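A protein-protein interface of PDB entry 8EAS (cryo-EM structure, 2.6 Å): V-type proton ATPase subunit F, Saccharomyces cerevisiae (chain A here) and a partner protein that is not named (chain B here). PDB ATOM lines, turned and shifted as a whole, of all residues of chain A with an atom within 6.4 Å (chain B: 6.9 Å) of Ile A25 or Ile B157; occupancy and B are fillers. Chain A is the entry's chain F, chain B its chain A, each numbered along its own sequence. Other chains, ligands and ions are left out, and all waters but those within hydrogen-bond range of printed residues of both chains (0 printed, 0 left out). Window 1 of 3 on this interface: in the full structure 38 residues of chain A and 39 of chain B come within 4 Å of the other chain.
Of the 24 printed residues of chain B, 10 touch a printed residue of chain A.
Printed residues of chain B that touch a printed residue of chain A: Tyr B69, Gly B71, Gln B72, Leu B73, Pro B132, Met B135, Phe B153, Lys B154, Ile B157 and Ile B160.
Hydrophobic or aromatic side chains of chain B within 4 Å of the printed part of chain A: Tyr B69, Leu B73, Pro B132, Met B135, Phe B153, Ile B157 and Ile B160.
Hydrophobic or aromatic side chains of chain A that line the printed part of chain B: Leu A21, Ala A23, Ile A25 and Leu A68.
Printed residues of chain B within 4 Å of Leu A21: Tyr B69 (3.8 Å), Pro B132 (3.0 Å) and Met B135 (3.8 Å).
Of chain B, only Tyr B69, Gly B71 and Ile B157 come within 4 Å of Ile A25.
Phe A37 touches none of the printed residues of chain B.
Printed residues of chain A within 4 Å of Tyr B69: Leu A21 (3.8 Å), Gly A24 (3.9 Å), Ile A25 (3.6 Å), Gly A26 (3.6 Å) and Gln A27 (2.7 Å).
Printed residues of chain A within 4 Å of Lys B154: Leu A22 and Ala A23.
Of chain A, only Ala A23 and Ile A25 come within 4 Å of Ile B157.
The nearest printed residue of chain A that does not touch Pro B132 is Ala A23 (4.6 Å).
Among the printed residues, merely in contact across the chains: Leu A21 with Pro B132 (3.0 Å), Gly A24 with Gly B71 (3.1 Å), Gly A26 with Gly B71 (3.2 Å), Ala A23 with Leu B73 (3.3 Å), Ala A23 with Ile B157 (3.5 Å), Leu A22 with Pro B132 (3.6 Å), Gly A26 with Tyr B69 (3.6 Å), Ile A25 with Tyr B69 (3.6 Å), Gly A24 with Pro B132 (3.7 Å), Ala A23 with Phe B153 (3.7 Å), Ala A23 with Lys B154 (3.7 Å), Leu A21 with Tyr B69 (3.8 Å), Leu A21 with Met B135 (3.8 Å), Ile A25 with Ile B157 (3.8 Å), Leu A68 with Ile B160 (3.8 Å), Leu A22 with Lys B154 (3.9 Å), Gly A24 with Tyr B69 (3.9 Å) and Ile A25 with Gly B71 (3.95 Å).
The backbone NH (N) of Gln A27 sits at hydrogen-bond distance from the backbone carbonyl oxygen (O) of Tyr B69 (2.7 Å).
The backbone NH of Leu B73 is in hydrogen-bond range of the backbone carbonyl oxygen of Gly A24, 3.3 Å away.
The backbone carbonyl oxygen (O) of Gly A24 is in hydrogen-bond range of the backbone NH (N) of Gln B72 (2.7 Å).
The backbone carbonyl oxygen of Leu A20 is in hydrogen-bond range of the backbone NH of Ile A25 (3.0 Å).
O of Ala A9 sits at hydrogen-bond distance from N of Leu A68 (2.7 Å).
O of Gly A26 lies close to OD1 of Asn A36 (2.8 Å).
The backbone carbonyl oxygen (O) of Gln A27 sits at hydrogen-bond distance from the backbone NH (N) of Asn A36 (2.9 Å).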
ATOM      1  N   ILE A   8       3.743  14.738   6.621  1.00  0.00           N
ATOM      2  CA  ILE A   8       2.429  15.369   6.646  1.00  0.00           C
ATOM      3  C   ILE A   8       1.834  15.265   5.250  1.00  0.00           C
ATOM      4  O   ILE A   8       2.413  15.768   4.281  1.00  0.00           O
ATOM      5  CB  ILE A   8       2.509  16.834   7.099  1.00  0.00           C
ATOM      6  CG1 ILE A   8       3.183  16.939   8.466  1.00  0.00           C
ATOM      7  CG2 ILE A   8       1.123  17.443   7.154  1.00  0.00           C
ATOM      8  CD1 ILE A   8       3.581  18.343   8.834  1.00  0.00           C
ATOM      9  N   ALA A   9       0.682  14.613   5.147  1.00  0.00           N
ATOM     10  CA  ALA A   9      -0.043  14.497   3.892  1.00  0.00           C
ATOM     11  C   ALA A   9      -1.188  15.497   3.867  1.00  0.00           C
ATOM     12  O   ALA A   9      -1.771  15.826   4.900  1.00  0.00           O
ATOM     13  CB  ALA A   9      -0.583  13.082   3.694  1.00  0.00           C
ATOM     14  N   VAL A  10      -1.496  15.993   2.674  1.00  0.00           N
ATOM     15  CA  VAL A  10      -2.494  17.036   2.500  1.00  0.00           C
ATOM     16  C   VAL A  10      -3.446  16.635   1.384  1.00  0.00           C
ATOM     17  O   VAL A  10      -3.008  16.284   0.284  1.00  0.00           O
ATOM     18  CB  VAL A  10      -1.844  18.398   2.191  1.00  0.00           C
ATOM     19  CG1 VAL A  10      -2.893  19.399   1.788  1.00  0.00           C
ATOM     20  CG2 VAL A  10      -1.074  18.901   3.396  1.00  0.00           C
ATOM     21  N   LEU A  20      -0.654  25.942   2.718  1.00  0.00           N
ATOM     22  CA  LEU A  20       0.105  24.949   3.468  1.00  0.00           C
ATOM     23  C   LEU A  20       1.536  24.845   2.962  1.00  0.00           C
ATOM     24  O   LEU A  20       2.456  24.589   3.744  1.00  0.00           O
ATOM     25  CB  LEU A  20      -0.593  23.595   3.399  1.00  0.00           C
ATOM     26  CG  LEU A  20      -1.902  23.553   4.186  1.00  0.00           C
ATOM     27  CD1 LEU A  20      -2.620  22.251   3.956  1.00  0.00           C
ATOM     28  CD2 LEU A  20      -1.653  23.775   5.661  1.00  0.00           C
ATOM     29  N   LEU A  21       1.744  25.030   1.658  1.00  0.00           N
ATOM     30  CA  LEU A  21       3.103  25.127   1.143  1.00  0.00           C
ATOM     31  C   LEU A  21       3.811  26.340   1.716  1.00  0.00           C
ATOM     32  O   LEU A  21       4.976  26.252   2.115  1.00  0.00           O
ATOM     33  CB  LEU A  21       3.095  25.192  -0.381  1.00  0.00           C
ATOM     34  CG  LEU A  21       2.901  23.881  -1.133  1.00  0.00           C
ATOM     35  CD1 LEU A  21       2.481  24.166  -2.554  1.00  0.00           C
ATOM     36  CD2 LEU A  21       4.172  23.060  -1.103  1.00  0.00           C
ATOM     37  N   LEU A  22       3.119  27.480   1.775  1.00  0.00           N
ATOM     38  CA  LEU A  22       3.703  28.667   2.390  1.00  0.00           C
ATOM     39  C   LEU A  22       4.035  28.414   3.852  1.00  0.00           C
ATOM     40  O   LEU A  22       5.014  28.953   4.378  1.00  0.00           O
ATOM     41  CB  LEU A  22       2.748  29.849   2.256  1.00  0.00           C
ATOM     42  CG  LEU A  22       2.694  30.547   0.901  1.00  0.00           C
ATOM     43  CD1 LEU A  22       1.522  31.503   0.873  1.00  0.00           C
ATOM     44  CD2 LEU A  22       3.989  31.272   0.618  1.00  0.00           C
ATOM     45  N   ALA A  23       3.227  27.595   4.525  1.00  0.00           N
ATOM     46  CA  ALA A  23       3.510  27.222   5.903  1.00  0.00           C
ATOM     47  C   ALA A  23       4.772  26.384   6.029  1.00  0.00           C
ATOM     48  O   ALA A  23       5.328  26.282   7.127  1.00  0.00           O
ATOM     49  CB  ALA A  23       2.327  26.460   6.487  1.00  0.00           C
ATOM     50  N   GLY A  24       5.234  25.780   4.940  1.00  0.00           N
ATOM     51  CA  GLY A  24       6.417  24.954   4.964  1.00  0.00           C
ATOM     52  C   GLY A  24       6.177  23.467   4.855  1.00  0.00           C
ATOM     53  O   GLY A  24       7.112  22.696   5.079  1.00  0.00           O
ATOM     54  N   ILE A  25       4.958  23.037   4.538  1.00  0.00           N
ATOM     55  CA  ILE A  25       4.694  21.617   4.343  1.00  0.00           C
ATOM     56  C   ILE A  25       5.186  21.193   2.967  1.00  0.00           C
ATOM     57  O   ILE A  25       5.038  21.924   1.979  1.00  0.00           O
ATOM     58  CB  ILE A  25       3.198  21.321   4.534  1.00  0.00           C
ATOM     59  CG1 ILE A  25       2.709  21.948   5.839  1.00  0.00           C
ATOM     60  CG2 ILE A  25       2.936  19.830   4.509  1.00  0.00           C
ATOM     61  CD1 ILE A  25       1.347  21.484   6.270  1.00  0.00           C
ATOM     62  N   GLY A  26       5.785  20.010   2.899  1.00  0.00           N
ATOM     63  CA  GLY A  26       6.482  19.585   1.706  1.00  0.00           C
ATOM     64  C   GLY A  26       5.619  18.806   0.735  1.00  0.00           C
ATOM     65  O   GLY A  26       4.691  18.108   1.119  1.00  0.00           O
ATOM     66  N   GLN A  27       5.960  18.936  -0.545  1.00  0.00           N
ATOM     67  CA  GLN A  27       5.203  18.272  -1.597  1.00  0.00           C
ATOM     68  C   GLN A  27       5.526  16.786  -1.676  1.00  0.00           C
ATOM     69  O   GLN A  27       4.634  15.971  -1.927  1.00  0.00           O
ATOM     70  CB  GLN A  27       5.484  18.948  -2.939  1.00  0.00           C
ATOM     71  CG  GLN A  27       4.518  20.054  -3.306  1.00  0.00           C
ATOM     72  CD  GLN A  27       3.238  19.530  -3.914  1.00  0.00           C
ATOM     73  OE1 GLN A  27       3.069  18.325  -4.089  1.00  0.00           O
ATOM     74  NE2 GLN A  27       2.331  20.436  -4.254  1.00  0.00           N
ATOM     75  N   ASN A  36       3.204  13.546  -1.443  1.00  0.00           N
ATOM     76  CA  ASN A  36       2.271  13.443  -0.329  1.00  0.00           C
ATOM     77  C   ASN A  36       1.293  14.612  -0.282  1.00  0.00           C
ATOM     78  O   ASN A  36       0.768  14.938   0.786  1.00  0.00           O
ATOM     79  CB  ASN A  36       3.028  13.281   0.994  1.00  0.00           C
ATOM     80  CG  ASN A  36       3.870  14.486   1.357  1.00  0.00           C
ATOM     81  OD1 ASN A  36       3.484  15.630   1.133  1.00  0.00           O
ATOM     82  ND2 ASN A  36       5.035  14.227   1.939  1.00  0.00           N
ATOM     83  N   PHE A  37       1.055  15.256  -1.418  1.00  0.00           N
ATOM     84  CA  PHE A  37      -0.016  16.223  -1.587  1.00  0.00           C
ATOM     85  C   PHE A  37      -1.014  15.700  -2.607  1.00  0.00           C
ATOM     86  O   PHE A  37      -0.635  15.099  -3.614  1.00  0.00           O
ATOM     87  CB  PHE A  37       0.512  17.577  -2.066  1.00  0.00           C
ATOM     88  CG  PHE A  37       0.756  18.564  -0.968  1.00  0.00           C
ATOM     89  CD1 PHE A  37       0.071  19.761  -0.943  1.00  0.00           C
ATOM     90  CD2 PHE A  37       1.675  18.308   0.028  1.00  0.00           C
ATOM     91  CE1 PHE A  37       0.294  20.679   0.057  1.00  0.00           C
ATOM     92  CE2 PHE A  37       1.898  19.224   1.031  1.00  0.00           C
ATOM     93  CZ  PHE A  37       1.211  20.410   1.044  1.00  0.00           C
ATOM     94  N   LEU A  68      -3.831  16.272   6.583  1.00  0.00           N
ATOM     95  CA  LEU A  68      -4.633  17.486   6.578  1.00  0.00           C
ATOM     96  C   LEU A  68      -5.581  17.444   5.389  1.00  0.00           C
ATOM     97  O   LEU A  68      -5.137  17.341   4.242  1.00  0.00           O
ATOM     98  CB  LEU A  68      -3.745  18.726   6.504  1.00  0.00           C
ATOM     99  CG  LEU A  68      -2.709  18.925   7.603  1.00  0.00           C
ATOM    100  CD1 LEU A  68      -1.924  20.192   7.343  1.00  0.00           C
ATOM    101  CD2 LEU A  68      -3.381  18.985   8.958  1.00  0.00           C
ATOM    102  N   LEU B  34      -7.249  28.680  14.962  1.00  0.00           N
ATOM    103  CA  LEU B  34      -6.944  28.104  13.660  1.00  0.00           C
ATOM    104  C   LEU B  34      -7.808  28.715  12.571  1.00  0.00           C
ATOM    105  O   LEU B  34      -7.324  28.993  11.469  1.00  0.00           O
ATOM    106  CB  LEU B  34      -7.141  26.591  13.693  1.00  0.00           C
ATOM    107  CG  LEU B  34      -6.579  25.862  12.474  1.00  0.00           C
ATOM    108  CD1 LEU B  34      -5.068  25.845  12.498  1.00  0.00           C
ATOM    109  CD2 LEU B  34      -7.137  24.461  12.366  1.00  0.00           C
ATOM    110  N   PHE B  38      -6.383  30.785   9.407  1.00  0.00           N
ATOM    111  CA  PHE B  38      -6.679  30.410   8.030  1.00  0.00           C
ATOM    112  C   PHE B  38      -7.416  31.517   7.293  1.00  0.00           C
ATOM    113  O   PHE B  38      -7.153  31.751   6.114  1.00  0.00           O
ATOM    114  CB  PHE B  38      -7.475  29.108   7.980  1.00  0.00           C
ATOM    115  CG  PHE B  38      -6.619  27.876   7.929  1.00  0.00           C
ATOM    116  CD1 PHE B  38      -6.072  27.454   6.736  1.00  0.00           C
ATOM    117  CD2 PHE B  38      -6.375  27.132   9.064  1.00  0.00           C
ATOM    118  CE1 PHE B  38      -5.291  26.324   6.677  1.00  0.00           C
ATOM    119  CE2 PHE B  38      -5.595  25.999   9.008  1.00  0.00           C
ATOM    120  CZ  PHE B  38      -5.053  25.597   7.815  1.00  0.00           C
ATOM    121  N   TYR B  69       9.565  20.144  -3.928  1.00  0.00           N
ATOM    122  CA  TYR B  69       9.793  20.860  -2.682  1.00  0.00           C
ATOM    123  C   TYR B  69       9.606  19.921  -1.502  1.00  0.00           C
ATOM    124  O   TYR B  69       8.506  19.405  -1.277  1.00  0.00           O
ATOM    125  CB  TYR B  69       8.844  22.050  -2.566  1.00  0.00           C
ATOM    126  CG  TYR B  69       8.963  22.786  -1.257  1.00  0.00           C
ATOM    127  CD1 TYR B  69      10.159  23.370  -0.881  1.00  0.00           C
ATOM    128  CD2 TYR B  69       7.887  22.884  -0.390  1.00  0.00           C
ATOM    129  CE1 TYR B  69      10.279  24.035   0.310  1.00  0.00           C
ATOM    130  CE2 TYR B  69       8.001  23.548   0.809  1.00  0.00           C
ATOM    131  CZ  TYR B  69       9.200  24.122   1.151  1.00  0.00           C
ATOM    132  OH  TYR B  69       9.334  24.789   2.342  1.00  0.00           O
ATOM    133  N   ILE B  70      10.674  19.697  -0.753  1.00  0.00           N
ATOM    134  CA  ILE B  70      10.583  19.061   0.553  1.00  0.00           C
ATOM    135  C   ILE B  70      10.449  20.168   1.588  1.00  0.00           C
ATOM    136  O   ILE B  70      11.167  21.174   1.537  1.00  0.00           O
ATOM    137  CB  ILE B  70      11.804  18.169   0.830  1.00  0.00           C
ATOM    138  CG1 ILE B  70      13.100  18.973   0.757  1.00  0.00           C
ATOM    139  CG2 ILE B  70      11.847  17.020  -0.159  1.00  0.00           C
ATOM    140  CD1 ILE B  70      14.301  18.226   1.268  1.00  0.00           C
ATOM    141  N   GLY B  71       9.517  20.003   2.505  1.00  0.00           N
ATOM    142  CA  GLY B  71       9.117  21.105   3.344  1.00  0.00           C
ATOM    143  C   GLY B  71      10.136  21.462   4.402  1.00  0.00           C
ATOM    144  O   GLY B  71      11.188  20.845   4.556  1.00  0.00           O
ATOM    145  N   GLN B  72       9.803  22.516   5.136  1.00  0.00           N
ATOM    146  CA  GLN B  72      10.567  22.919   6.301  1.00  0.00           C
ATOM    147  C   GLN B  72      10.100  22.232   7.574  1.00  0.00           C
ATOM    148  O   GLN B  72      10.721  22.425   8.623  1.00  0.00           O
ATOM    149  CB  GLN B  72      10.469  24.433   6.478  1.00  0.00           C
ATOM    150  CG  GLN B  72      11.067  25.221   5.342  1.00  0.00           C
ATOM    151  CD  GLN B  72      11.348  26.648   5.727  1.00  0.00           C
ATOM    152  OE1 GLN B  72      12.458  27.145   5.548  1.00  0.00           O
ATOM    153  NE2 GLN B  72      10.340  27.321   6.264  1.00  0.00           N
ATOM    154  N   LEU B  73       9.032  21.443   7.510  1.00  0.00           N
ATOM    155  CA  LEU B  73       8.396  20.884   8.693  1.00  0.00           C
ATOM    156  C   LEU B  73       8.235  19.378   8.559  1.00  0.00           C
ATOM    157  O   LEU B  73       8.011  18.853   7.466  1.00  0.00           O
ATOM    158  CB  LEU B  73       7.016  21.506   8.932  1.00  0.00           C
ATOM    159  CG  LEU B  73       6.903  23.026   8.935  1.00  0.00           C
ATOM    160  CD1 LEU B  73       5.452  23.430   8.798  1.00  0.00           C
ATOM    161  CD2 LEU B  73       7.498  23.592  10.206  1.00  0.00           C
ATOM    162  N   GLU B  87       3.458  16.132  17.066  1.00  0.00           N
ATOM    163  CA  GLU B  87       4.042  17.464  17.081  1.00  0.00           C
ATOM    164  C   GLU B  87       4.699  17.755  15.741  1.00  0.00           C
ATOM    165  O   GLU B  87       5.329  16.878  15.146  1.00  0.00           O
ATOM    166  CB  GLU B  87       5.073  17.600  18.206  1.00  0.00           C
ATOM    167  CG  GLU B  87       5.702  18.978  18.320  1.00  0.00           C
ATOM    168  CD  GLU B  87       4.684  20.056  18.627  1.00  0.00           C
ATOM    169  OE1 GLU B  87       4.090  20.014  19.724  1.00  0.00           O
ATOM    170  OE2 GLU B  87       4.481  20.948  17.778  1.00  0.00           O
ATOM    171  N   ILE B  88       4.548  18.990  15.272  1.00  0.00           N
ATOM    172  CA  ILE B  88       5.173  19.450  14.039  1.00  0.00           C
ATOM    173  C   ILE B  88       6.393  20.283  14.404  1.00  0.00           C
ATOM    174  O   ILE B  88       6.285  21.256  15.158  1.00  0.00           O
ATOM    175  CB  ILE B  88       4.188  20.261  13.181  1.00  0.00           C
ATOM    176  CG1 ILE B  88       2.958  19.421  12.847  1.00  0.00           C
ATOM    177  CG2 ILE B  88       4.864  20.736  11.912  1.00  0.00           C
ATOM    178  CD1 ILE B  88       1.790  20.229  12.346  1.00  0.00           C
ATOM    179  N   VAL B  89       7.553  19.906  13.865  1.00  0.00           N
ATOM    180  CA  VAL B  89       8.813  20.556  14.190  1.00  0.00           C
ATOM    181  C   VAL B  89       9.451  21.077  12.909  1.00  0.00           C
ATOM    182  O   VAL B  89       9.119  20.654  11.801  1.00  0.00           O
ATOM    183  CB  VAL B  89       9.786  19.614  14.929  1.00  0.00           C
ATOM    184  CG1 VAL B  89       9.097  18.953  16.106  1.00  0.00           C
ATOM    185  CG2 VAL B  89      10.335  18.572  13.979  1.00  0.00           C
ATOM    186  N   PRO B 132       9.518  28.881   1.851  1.00  0.00           N
ATOM    187  CA  PRO B 132       8.520  28.607   0.807  1.00  0.00           C
ATOM    188  C   PRO B 132       8.126  29.821  -0.003  1.00  0.00           C
ATOM    189  O   PRO B 132       7.539  29.660  -1.077  1.00  0.00           O
ATOM    190  CB  PRO B 132       7.327  28.069   1.599  1.00  0.00           C
ATOM    191  CG  PRO B 132       7.903  27.537   2.832  1.00  0.00           C
ATOM    192  CD  PRO B 132       9.069  28.402   3.168  1.00  0.00           C
ATOM    193  N   MET B 135       9.327  29.757  -3.563  1.00  0.00           N
ATOM    194  CA  MET B 135       8.552  29.022  -4.557  1.00  0.00           C
ATOM    195  C   MET B 135       7.805  29.969  -5.479  1.00  0.00           C
ATOM    196  O   MET B 135       7.641  29.685  -6.669  1.00  0.00           O
ATOM    197  CB  MET B 135       7.548  28.115  -3.851  1.00  0.00           C
ATOM    198  CG  MET B 135       8.134  26.987  -3.050  1.00  0.00           C
ATOM    199  SD  MET B 135       6.827  26.091  -2.203  1.00  0.00           S
ATOM    200  CE  MET B 135       6.022  25.285  -3.564  1.00  0.00           C
ATOM    201  N   SER B 152       0.572  34.028   8.426  1.00  0.00           N
ATOM    202  CA  SER B 152      -0.673  33.514   8.987  1.00  0.00           C
ATOM    203  C   SER B 152      -0.718  31.991   8.934  1.00  0.00           C
ATOM    204  O   SER B 152      -1.138  31.339   9.897  1.00  0.00           O
ATOM    205  CB  SER B 152      -1.858  34.119   8.246  1.00  0.00           C
ATOM    206  OG  SER B 152      -1.765  35.530   8.226  1.00  0.00           O
ATOM    207  N   PHE B 153      -0.271  31.400   7.828  1.00  0.00           N
ATOM    208  CA  PHE B 153      -0.308  29.942   7.725  1.00  0.00           C
ATOM    209  C   PHE B 153       0.756  29.287   8.607  1.00  0.00           C
ATOM    210  O   PHE B 153       0.519  28.224   9.206  1.00  0.00           O
ATOM    211  CB  PHE B 153      -0.150  29.531   6.265  1.00  0.00           C
ATOM    212  CG  PHE B 153      -1.364  29.815   5.433  1.00  0.00           C
ATOM    213  CD1 PHE B 153      -2.558  29.169   5.688  1.00  0.00           C
ATOM    214  CD2 PHE B 153      -1.317  30.733   4.404  1.00  0.00           C
ATOM    215  CE1 PHE B 153      -3.674  29.430   4.930  1.00  0.00           C
ATOM    216  CE2 PHE B 153      -2.433  30.997   3.647  1.00  0.00           C
ATOM    217  CZ  PHE B 153      -3.609  30.344   3.909  1.00  0.00           C
ATOM    218  N   LYS B 154       1.932  29.907   8.705  1.00  0.00           N
ATOM    219  CA  LYS B 154       2.955  29.401   9.609  1.00  0.00           C
ATOM    220  C   LYS B 154       2.491  29.485  11.052  1.00  0.00           C
ATOM    221  O   LYS B 154       2.916  28.687  11.893  1.00  0.00           O
ATOM    222  CB  LYS B 154       4.259  30.171   9.420  1.00  0.00           C
ATOM    223  CG  LYS B 154       4.999  29.838   8.148  1.00  0.00           C
ATOM    224  CD  LYS B 154       6.116  30.826   7.900  1.00  0.00           C
ATOM    225  CE  LYS B 154       7.307  30.542   8.793  1.00  0.00           C
ATOM    226  NZ  LYS B 154       8.324  29.702   8.102  1.00  0.00           N
ATOM    227  N   GLY B 155       1.638  30.459  11.364  1.00  0.00           N
ATOM    228  CA  GLY B 155       1.004  30.479  12.670  1.00  0.00           C
ATOM    229  C   GLY B 155      -0.071  29.424  12.810  1.00  0.00           C
ATOM    230  O   GLY B 155      -0.332  28.940  13.912  1.00  0.00           O
ATOM    231  N   CYS B 156      -0.720  29.070  11.700  1.00  0.00           N
ATOM    232  CA  CYS B 156      -1.704  27.990  11.723  1.00  0.00           C
ATOM    233  C   CYS B 156      -1.064  26.660  12.094  1.00  0.00           C
ATOM    234  O   CYS B 156      -1.700  25.817  12.735  1.00  0.00           O
ATOM    235  CB  CYS B 156      -2.395  27.871  10.367  1.00  0.00           C
ATOM    236  SG  CYS B 156      -3.517  29.199   9.971  1.00  0.00           S
ATOM    237  N   ILE B 157       0.180  26.440  11.667  1.00  0.00           N
ATOM    238  CA  ILE B 157       0.828  25.141  11.910  1.00  0.00           C
ATOM    239  C   ILE B 157       0.879  24.758  13.389  1.00  0.00           C
ATOM    240  O   ILE B 157       0.461  23.636  13.727  1.00  0.00           O
ATOM    241  CB  ILE B 157       2.217  25.110  11.247  1.00  0.00           C
ATOM    242  CG1 ILE B 157       2.086  25.189   9.731  1.00  0.00           C
ATOM    243  CG2 ILE B 157       2.964  23.856  11.643  1.00  0.00           C
ATOM    244  CD1 ILE B 157       1.338  24.027   9.128  1.00  0.00           C
ATOM    245  N   PRO B 158       1.370  25.604  14.310  1.00  0.00           N
ATOM    246  CA  PRO B 158       1.294  25.226  15.732  1.00  0.00           C
ATOM    247  C   PRO B 158      -0.124  24.992  16.202  1.00  0.00           C
ATOM    248  O   PRO B 158      -0.367  24.118  17.041  1.00  0.00           O
ATOM    249  CB  PRO B 158       1.935  26.420  16.450  1.00  0.00           C
ATOM    250  CG  PRO B 158       2.778  27.067  15.443  1.00  0.00           C
ATOM    251  CD  PRO B 158       2.077  26.884  14.140  1.00  0.00           C
ATOM    252  N   LEU B 159      -1.075  25.764  15.679  1.00  0.00           N
ATOM    253  CA  LEU B 159      -2.471  25.547  16.023  1.00  0.00           C
ATOM    254  C   LEU B 159      -2.961  24.211  15.484  1.00  0.00           C
ATOM    255  O   LEU B 159      -3.775  23.542  16.123  1.00  0.00           O
ATOM    256  CB  LEU B 159      -3.323  26.695  15.494  1.00  0.00           C
ATOM    257  CG  LEU B 159      -2.932  28.048  16.084  1.00  0.00           C
ATOM    258  CD1 LEU B 159      -3.590  29.177  15.317  1.00  0.00           C
ATOM    259  CD2 LEU B 159      -3.289  28.101  17.557  1.00  0.00           C
ATOM    260  N   ILE B 160      -2.467  23.801  14.314  1.00  0.00           N
ATOM    261  CA  ILE B 160      -2.807  22.481  13.789  1.00  0.00           C
ATOM    262  C   ILE B 160      -2.320  21.398  14.739  1.00  0.00           C
ATOM    263  O   ILE B 160      -3.055  20.458  15.073  1.00  0.00           O
ATOM    264  CB  ILE B 160      -2.221  22.291  12.378  1.00  0.00           C
ATOM    265  CG1 ILE B 160      -3.103  22.961  11.328  1.00  0.00           C
ATOM    266  CG2 ILE B 160      -2.069  20.816  12.060  1.00  0.00           C
ATOM    267  CD1 ILE B 160      -2.423  23.126   9.988  1.00  0.00           C
ATOM    268  N   ALA B 161      -1.071  21.514  15.193  1.00  0.00           N
ATOM    269  CA  ALA B 161      -0.527  20.508  16.102  1.00  0.00           C
ATOM    270  C   ALA B 161      -1.305  20.472  17.412  1.00  0.00           C
ATOM    271  O   ALA B 161      -1.661  19.395  17.910  1.00  0.00           O
ATOM    272  CB  ALA B 161       0.955  20.778  16.359  1.00  0.00           C
ATOM    273  N   GLN B 162      -1.587  21.647  17.980  1.00  0.00           N
ATOM    274  CA  GLN B 162      -2.333  21.706  19.232  1.00  0.00           C
ATOM    275  C   GLN B 162      -3.736  21.142  19.066  1.00  0.00           C
ATOM    276  O   GLN B 162      -4.242  20.452  19.955  1.00  0.00           O
ATOM    277  CB  GLN B 162      -2.396  23.144  19.741  1.00  0.00           C
ATOM    278  CG  GLN B 162      -1.059  23.704  20.171  1.00  0.00           C
ATOM    279  CD  GLN B 162      -1.159  25.129  20.663  1.00  0.00           C
ATOM    280  OE1 GLN B 162      -2.229  25.734  20.633  1.00  0.00           O
ATOM    281  NE2 GLN B 162      -0.038  25.679  21.114  1.00  0.00           N
ATOM    282  N   LEU B 163      -4.384  21.435  17.940  1.00  0.00           N
ATOM    283  CA  LEU B 163      -5.723  20.922  17.689  1.00  0.00           C
ATOM    284  C   LEU B 163      -5.724  19.407  17.570  1.00  0.00           C
ATOM    285  O   LEU B 163      -6.614  18.741  18.105  1.00  0.00           O
ATOM    286  CB  LEU B 163      -6.285  21.561  16.423  1.00  0.00           C
ATOM    287  CG  LEU B 163      -7.799  21.567  16.262  1.00  0.00           C
ATOM    288  CD1 LEU B 163      -8.439  22.359  17.374  1.00  0.00           C
ATOM    289  CD2 LEU B 163      -8.145  22.157  14.920  1.00  0.00           C
